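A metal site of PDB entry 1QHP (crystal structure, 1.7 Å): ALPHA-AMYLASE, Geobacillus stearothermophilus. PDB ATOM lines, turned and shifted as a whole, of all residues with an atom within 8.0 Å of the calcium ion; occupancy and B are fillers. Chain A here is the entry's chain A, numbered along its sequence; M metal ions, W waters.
OD1 of Asn 27 is bound to the calcium ion (2.5 Å). OD2 of Asp 50 binds the calcium ion, at 2.5 Å. OD1 of Asp 21 is bound to the calcium ion. The calcium ion is bound by O of Gly 48. The calcium ion is bound by the side-chain amide oxygen (OD1) of Asn 26 (2.6 Å). The backbone carbonyl oxygen (O) of Asp 23 is bound to the calcium ion, at 2.6 Å. Water W1 binds the calcium ion (2.6 Å). The calcium ion has seven donor atoms within binding distance.
O of Thr 24 sits close to OD1 of Asn 27. A ring nitrogen (NE2) of His 103 sits close to the backbone carbonyl oxygen of Asn 27 (3.4 Å). The side-chain amide nitrogen of Asn 27 lies within hydrogen-bond range of the side-chain hydroxyl of Tyr 36, 3.2 Å away. The side-chain carboxylate (OD1) of Asp 50 lies within hydrogen-bond range of the backbone NH (N) of Gly 22 (2.8 Å). The backbone NH (N) of Asp 50 is in hydrogen-bond range of the backbone carbonyl oxygen (O) of Tyr 20. OD1 of Asp 50 is in hydrogen-bond range of N of Gly 53 (2.8 Å). ND2 of Asn 26 lies close to O of His 103 (3.4 Å). OD1 of Asp 23 sits at hydrogen-bond distance from OG1 of Thr 25 (2.7 Å).
Of the 23 residues printed, 6 come within 4 Å of the calcium ion. The nearest printed residue that does not touch the calcium ion is Thr 24 (4.3 Å).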
ATOM      1  N   ILE A  16      24.400  25.209 -20.660  1.00  0.00           N
ATOM      2  CA  ILE A  16      24.385  25.725 -19.297  1.00  0.00           C
ATOM      3  C   ILE A  16      25.403  25.112 -18.367  1.00  0.00           C
ATOM      4  O   ILE A  16      26.121  25.848 -17.662  1.00  0.00           O
ATOM      5  CB  ILE A  16      22.979  25.591 -18.688  1.00  0.00           C
ATOM      6  CG1 ILE A  16      21.985  26.473 -19.460  1.00  0.00           C
ATOM      7  CG2 ILE A  16      22.946  25.940 -17.195  1.00  0.00           C
ATOM      8  CD1 ILE A  16      20.545  26.096 -19.189  1.00  0.00           C
ATOM      9  N   ASP A  17      25.506  23.788 -18.332  1.00  0.00           N
ATOM     10  CA  ASP A  17      26.445  23.174 -17.381  1.00  0.00           C
ATOM     11  C   ASP A  17      27.897  23.510 -17.612  1.00  0.00           C
ATOM     12  O   ASP A  17      28.739  23.357 -16.709  1.00  0.00           O
ATOM     13  CB  ASP A  17      26.242  21.642 -17.479  1.00  0.00           C
ATOM     14  CG  ASP A  17      27.124  20.911 -16.468  1.00  0.00           C
ATOM     15  OD1 ASP A  17      26.875  21.106 -15.269  1.00  0.00           O
ATOM     16  OD2 ASP A  17      28.052  20.203 -16.915  1.00  0.00           O
ATOM     17  N   TYR A  20      29.111  28.901 -16.862  1.00  0.00           N
ATOM     18  CA  TYR A  20      29.634  29.517 -15.643  1.00  0.00           C
ATOM     19  C   TYR A  20      28.891  29.013 -14.403  1.00  0.00           C
ATOM     20  O   TYR A  20      27.663  29.001 -14.365  1.00  0.00           O
ATOM     21  CB  TYR A  20      29.520  31.053 -15.721  1.00  0.00           C
ATOM     22  CG  TYR A  20      30.366  31.732 -14.653  1.00  0.00           C
ATOM     23  CD1 TYR A  20      31.743  31.660 -14.695  1.00  0.00           C
ATOM     24  CD2 TYR A  20      29.747  32.424 -13.624  1.00  0.00           C
ATOM     25  CE1 TYR A  20      32.522  32.277 -13.714  1.00  0.00           C
ATOM     26  CE2 TYR A  20      30.524  33.056 -12.658  1.00  0.00           C
ATOM     27  CZ  TYR A  20      31.897  32.977 -12.707  1.00  0.00           C
ATOM     28  OH  TYR A  20      32.656  33.594 -11.734  1.00  0.00           O
ATOM     29  N   ASP A  21      29.681  28.610 -13.419  1.00  0.00           N
ATOM     30  CA  ASP A  21      29.098  28.097 -12.162  1.00  0.00           C
ATOM     31  C   ASP A  21      28.850  29.301 -11.256  1.00  0.00           C
ATOM     32  O   ASP A  21      29.744  29.748 -10.526  1.00  0.00           O
ATOM     33  CB  ASP A  21      30.084  27.098 -11.584  1.00  0.00           C
ATOM     34  CG  ASP A  21      29.669  26.399 -10.319  1.00  0.00           C
ATOM     35  OD1 ASP A  21      28.557  26.700  -9.869  1.00  0.00           O
ATOM     36  OD2 ASP A  21      30.417  25.581  -9.727  1.00  0.00           O
ATOM     37  N   GLY A  22      27.631  29.855 -11.302  1.00  0.00           N
ATOM     38  CA  GLY A  22      27.334  31.056 -10.511  1.00  0.00           C
ATOM     39  C   GLY A  22      26.868  30.754  -9.088  1.00  0.00           C
ATOM     40  O   GLY A  22      26.696  31.652  -8.250  1.00  0.00           O
ATOM     41  N   ASP A  23      26.608  29.487  -8.801  1.00  0.00           N
ATOM     42  CA  ASP A  23      26.107  29.066  -7.494  1.00  0.00           C
ATOM     43  C   ASP A  23      26.716  27.707  -7.192  1.00  0.00           C
ATOM     44  O   ASP A  23      26.158  26.743  -7.715  1.00  0.00           O
ATOM     45  CB  ASP A  23      24.573  28.977  -7.517  1.00  0.00           C
ATOM     46  CG  ASP A  23      23.980  28.603  -6.159  1.00  0.00           C
ATOM     47  OD1 ASP A  23      24.750  28.266  -5.239  1.00  0.00           O
ATOM     48  OD2 ASP A  23      22.744  28.636  -6.012  1.00  0.00           O
ATOM     49  N   THR A  24      27.765  27.557  -6.414  1.00  0.00           N
ATOM     50  CA  THR A  24      28.336  26.225  -6.172  1.00  0.00           C
ATOM     51  C   THR A  24      27.464  25.339  -5.307  1.00  0.00           C
ATOM     52  O   THR A  24      27.677  24.114  -5.259  1.00  0.00           O
ATOM     53  CB  THR A  24      29.730  26.359  -5.516  1.00  0.00           C
ATOM     54  OG1 THR A  24      29.554  27.018  -4.242  1.00  0.00           O
ATOM     55  CG2 THR A  24      30.678  27.170  -6.393  1.00  0.00           C
ATOM     56  N   THR A  25      26.399  25.861  -4.687  1.00  0.00           N
ATOM     57  CA  THR A  25      25.555  25.114  -3.787  1.00  0.00           C
ATOM     58  C   THR A  25      24.590  24.169  -4.510  1.00  0.00           C
ATOM     59  O   THR A  25      24.080  23.279  -3.832  1.00  0.00           O
ATOM     60  CB  THR A  25      24.717  25.949  -2.789  1.00  0.00           C
ATOM     61  OG1 THR A  25      23.655  26.649  -3.424  1.00  0.00           O
ATOM     62  CG2 THR A  25      25.628  26.920  -2.055  1.00  0.00           C
ATOM     63  N   ASN A  26      24.398  24.322  -5.822  1.00  0.00           N
ATOM     64  CA  ASN A  26      23.499  23.361  -6.479  1.00  0.00           C
ATOM     65  C   ASN A  26      24.312  22.373  -7.312  1.00  0.00           C
ATOM     66  O   ASN A  26      23.725  21.690  -8.149  1.00  0.00           O
ATOM     67  CB  ASN A  26      22.457  24.104  -7.310  1.00  0.00           C
ATOM     68  CG  ASN A  26      23.049  25.032  -8.346  1.00  0.00           C
ATOM     69  OD1 ASN A  26      24.194  24.818  -8.704  1.00  0.00           O
ATOM     70  ND2 ASN A  26      22.369  26.060  -8.858  1.00  0.00           N
ATOM     71  N   ASN A  27      25.619  22.257  -7.074  1.00  0.00           N
ATOM     72  CA  ASN A  27      26.466  21.374  -7.867  1.00  0.00           C
ATOM     73  C   ASN A  27      26.180  19.890  -7.687  1.00  0.00           C
ATOM     74  O   ASN A  27      26.329  19.117  -8.638  1.00  0.00           O
ATOM     75  CB  ASN A  27      27.973  21.588  -7.552  1.00  0.00           C
ATOM     76  CG  ASN A  27      28.497  22.860  -8.162  1.00  0.00           C
ATOM     77  OD1 ASN A  27      27.664  23.602  -8.648  1.00  0.00           O
ATOM     78  ND2 ASN A  27      29.756  23.233  -8.194  1.00  0.00           N
ATOM     79  N   ASN A  28      25.750  19.488  -6.495  1.00  0.00           N
ATOM     80  CA  ASN A  28      25.528  18.061  -6.235  1.00  0.00           C
ATOM     81  C   ASN A  28      24.392  17.894  -5.241  1.00  0.00           C
ATOM     82  O   ASN A  28      24.567  17.540  -4.072  1.00  0.00           O
ATOM     83  CB  ASN A  28      26.867  17.546  -5.693  1.00  0.00           C
ATOM     84  CG  ASN A  28      26.969  16.030  -5.631  1.00  0.00           C
ATOM     85  OD1 ASN A  28      26.241  15.323  -6.318  1.00  0.00           O
ATOM     86  ND2 ASN A  28      27.890  15.553  -4.794  1.00  0.00           N
ATOM     87  N   TYR A  36      28.039  14.788 -10.180  1.00  0.00           N
ATOM     88  CA  TYR A  36      28.895  15.960 -10.313  1.00  0.00           C
ATOM     89  C   TYR A  36      30.369  15.598 -10.310  1.00  0.00           C
ATOM     90  O   TYR A  36      30.809  14.786  -9.497  1.00  0.00           O
ATOM     91  CB  TYR A  36      28.593  16.909  -9.148  1.00  0.00           C
ATOM     92  CG  TYR A  36      29.557  18.050  -8.920  1.00  0.00           C
ATOM     93  CD1 TYR A  36      29.771  19.026  -9.875  1.00  0.00           C
ATOM     94  CD2 TYR A  36      30.253  18.148  -7.718  1.00  0.00           C
ATOM     95  CE1 TYR A  36      30.651  20.082  -9.640  1.00  0.00           C
ATOM     96  CE2 TYR A  36      31.125  19.183  -7.488  1.00  0.00           C
ATOM     97  CZ  TYR A  36      31.320  20.145  -8.435  1.00  0.00           C
ATOM     98  OH  TYR A  36      32.204  21.183  -8.198  1.00  0.00           O
ATOM     99  N   TRP A  47      29.386  19.480 -14.604  1.00  0.00           N
ATOM    100  CA  TRP A  47      30.563  20.221 -14.183  1.00  0.00           C
ATOM    101  C   TRP A  47      30.178  21.431 -13.316  1.00  0.00           C
ATOM    102  O   TRP A  47      31.031  22.065 -12.698  1.00  0.00           O
ATOM    103  CB  TRP A  47      31.461  20.614 -15.353  1.00  0.00           C
ATOM    104  CG  TRP A  47      32.189  19.443 -15.963  1.00  0.00           C
ATOM    105  CD1 TRP A  47      32.173  18.144 -15.591  1.00  0.00           C
ATOM    106  CD2 TRP A  47      33.079  19.534 -17.074  1.00  0.00           C
ATOM    107  NE1 TRP A  47      32.961  17.392 -16.427  1.00  0.00           N
ATOM    108  CE2 TRP A  47      33.548  18.225 -17.340  1.00  0.00           C
ATOM    109  CE3 TRP A  47      33.510  20.594 -17.905  1.00  0.00           C
ATOM    110  CZ2 TRP A  47      34.423  17.953 -18.386  1.00  0.00           C
ATOM    111  CZ3 TRP A  47      34.397  20.303 -18.921  1.00  0.00           C
ATOM    112  CH2 TRP A  47      34.856  19.003 -19.146  1.00  0.00           C
ATOM    113  N   GLY A  48      28.885  21.783 -13.293  1.00  0.00           N
ATOM    114  CA  GLY A  48      28.441  22.819 -12.395  1.00  0.00           C
ATOM    115  C   GLY A  48      27.972  24.136 -12.961  1.00  0.00           C
ATOM    116  O   GLY A  48      27.511  24.976 -12.150  1.00  0.00           O
ATOM    117  N   GLY A  49      27.995  24.403 -14.246  1.00  0.00           N
ATOM    118  CA  GLY A  49      27.460  25.677 -14.766  1.00  0.00           C
ATOM    119  C   GLY A  49      25.966  25.713 -14.509  1.00  0.00           C
ATOM    120  O   GLY A  49      25.257  24.701 -14.539  1.00  0.00           O
ATOM    121  N   ASP A  50      25.418  26.933 -14.327  1.00  0.00           N
ATOM    122  CA  ASP A  50      23.995  27.013 -14.010  1.00  0.00           C
ATOM    123  C   ASP A  50      23.347  28.311 -14.492  1.00  0.00           C
ATOM    124  O   ASP A  50      23.987  29.128 -15.146  1.00  0.00           O
ATOM    125  CB  ASP A  50      23.842  26.859 -12.483  1.00  0.00           C
ATOM    126  CG  ASP A  50      24.808  27.802 -11.773  1.00  0.00           C
ATOM    127  OD1 ASP A  50      25.097  28.918 -12.201  1.00  0.00           O
ATOM    128  OD2 ASP A  50      25.363  27.418 -10.738  1.00  0.00           O
ATOM    129  N   LEU A  51      22.059  28.466 -14.208  1.00  0.00           N
ATOM    130  CA  LEU A  51      21.325  29.650 -14.665  1.00  0.00           C
ATOM    131  C   LEU A  51      21.813  30.917 -13.996  1.00  0.00           C
ATOM    132  O   LEU A  51      21.928  31.957 -14.667  1.00  0.00           O
ATOM    133  CB  LEU A  51      19.830  29.492 -14.396  1.00  0.00           C
ATOM    134  CG  LEU A  51      19.195  28.321 -15.184  1.00  0.00           C
ATOM    135  CD1 LEU A  51      17.788  28.103 -14.637  1.00  0.00           C
ATOM    136  CD2 LEU A  51      19.167  28.616 -16.678  1.00  0.00           C
ATOM    137  N   GLU A  52      22.175  30.846 -12.725  1.00  0.00           N
ATOM    138  CA  GLU A  52      22.740  32.039 -12.054  1.00  0.00           C
ATOM    139  C   GLU A  52      24.067  32.436 -12.670  1.00  0.00           C
ATOM    140  O   GLU A  52      24.383  33.628 -12.806  1.00  0.00           O
ATOM    141  CB  GLU A  52      22.804  31.751 -10.567  1.00  0.00           C
ATOM    142  CG  GLU A  52      23.415  32.810  -9.676  1.00  0.00           C
ATOM    143  CD  GLU A  52      22.833  34.204  -9.811  1.00  0.00           C
ATOM    144  OE1 GLU A  52      21.673  34.374 -10.251  1.00  0.00           O
ATOM    145  OE2 GLU A  52      23.596  35.113  -9.456  1.00  0.00           O
ATOM    146  N   GLY A  53      24.866  31.485 -13.166  1.00  0.00           N
ATOM    147  CA  GLY A  53      26.126  31.775 -13.836  1.00  0.00           C
ATOM    148  C   GLY A  53      25.883  32.521 -15.144  1.00  0.00           C
ATOM    149  O   GLY A  53      26.616  33.468 -15.455  1.00  0.00           O
ATOM    150  N   GLU A 102      17.435  20.818 -11.124  1.00  0.00           N
ATOM    151  CA  GLU A 102      17.937  21.278  -9.833  1.00  0.00           C
ATOM    152  C   GLU A 102      19.407  21.636  -9.832  1.00  0.00           C
ATOM    153  O   GLU A 102      19.821  22.532  -9.077  1.00  0.00           O
ATOM    154  CB  GLU A 102      17.631  20.267  -8.706  1.00  0.00           C
ATOM    155  CG  GLU A 102      18.420  18.964  -8.762  1.00  0.00           C
ATOM    156  CD  GLU A 102      17.908  17.988  -9.774  1.00  0.00           C
ATOM    157  OE1 GLU A 102      16.817  18.165 -10.391  1.00  0.00           O
ATOM    158  OE2 GLU A 102      18.584  16.948  -9.992  1.00  0.00           O
ATOM    159  N   HIS A 103      20.248  21.068 -10.707  1.00  0.00           N
ATOM    160  CA  HIS A 103      21.631  21.485 -10.826  1.00  0.00           C
ATOM    161  C   HIS A 103      21.718  22.916 -11.374  1.00  0.00           C
ATOM    162  O   HIS A 103      22.730  23.583 -11.141  1.00  0.00           O
ATOM    163  CB  HIS A 103      22.394  20.584 -11.811  1.00  0.00           C
ATOM    164  CG  HIS A 103      22.790  19.256 -11.217  1.00  0.00           C
ATOM    165  ND1 HIS A 103      21.962  18.149 -11.247  1.00  0.00           N
ATOM    166  CD2 HIS A 103      23.930  18.869 -10.606  1.00  0.00           C
ATOM    167  CE1 HIS A 103      22.589  17.137 -10.652  1.00  0.00           C
ATOM    168  NE2 HIS A 103      23.787  17.553 -10.269  1.00  0.00           N
ATOM    169  N   PHE A 104      20.690  23.365 -12.103  1.00  0.00           N
ATOM    170  CA  PHE A 104      20.729  24.680 -12.718  1.00  0.00           C
ATOM    171  C   PHE A 104      20.005  25.784 -11.959  1.00  0.00           C
ATOM    172  O   PHE A 104      20.330  26.954 -12.214  1.00  0.00           O
ATOM    173  CB  PHE A 104      20.174  24.598 -14.140  1.00  0.00           C
ATOM    174  CG  PHE A 104      20.850  23.632 -15.077  1.00  0.00           C
ATOM    175  CD1 PHE A 104      22.109  23.117 -14.842  1.00  0.00           C
ATOM    176  CD2 PHE A 104      20.218  23.287 -16.268  1.00  0.00           C
ATOM    177  CE1 PHE A 104      22.719  22.233 -15.718  1.00  0.00           C
ATOM    178  CE2 PHE A 104      20.813  22.416 -17.166  1.00  0.00           C
ATOM    179  CZ  PHE A 104      22.062  21.885 -16.894  1.00  0.00           C
ATOM    180  N   GLY A 105      19.090  25.434 -11.079  1.00  0.00           N
ATOM    181  CA  GLY A 105      18.391  26.453 -10.282  1.00  0.00           C
ATOM    182  C   GLY A 105      16.956  25.984 -10.052  1.00  0.00           C
ATOM    183  O   GLY A 105      16.682  24.782 -10.141  1.00  0.00           O
HETATM  184 CA    CA M   1      26.411  25.333  -9.872  1.00  0.00          CA
HETATM  185  O   HOH W   1      25.323  23.218 -10.942  1.00  0.00           O
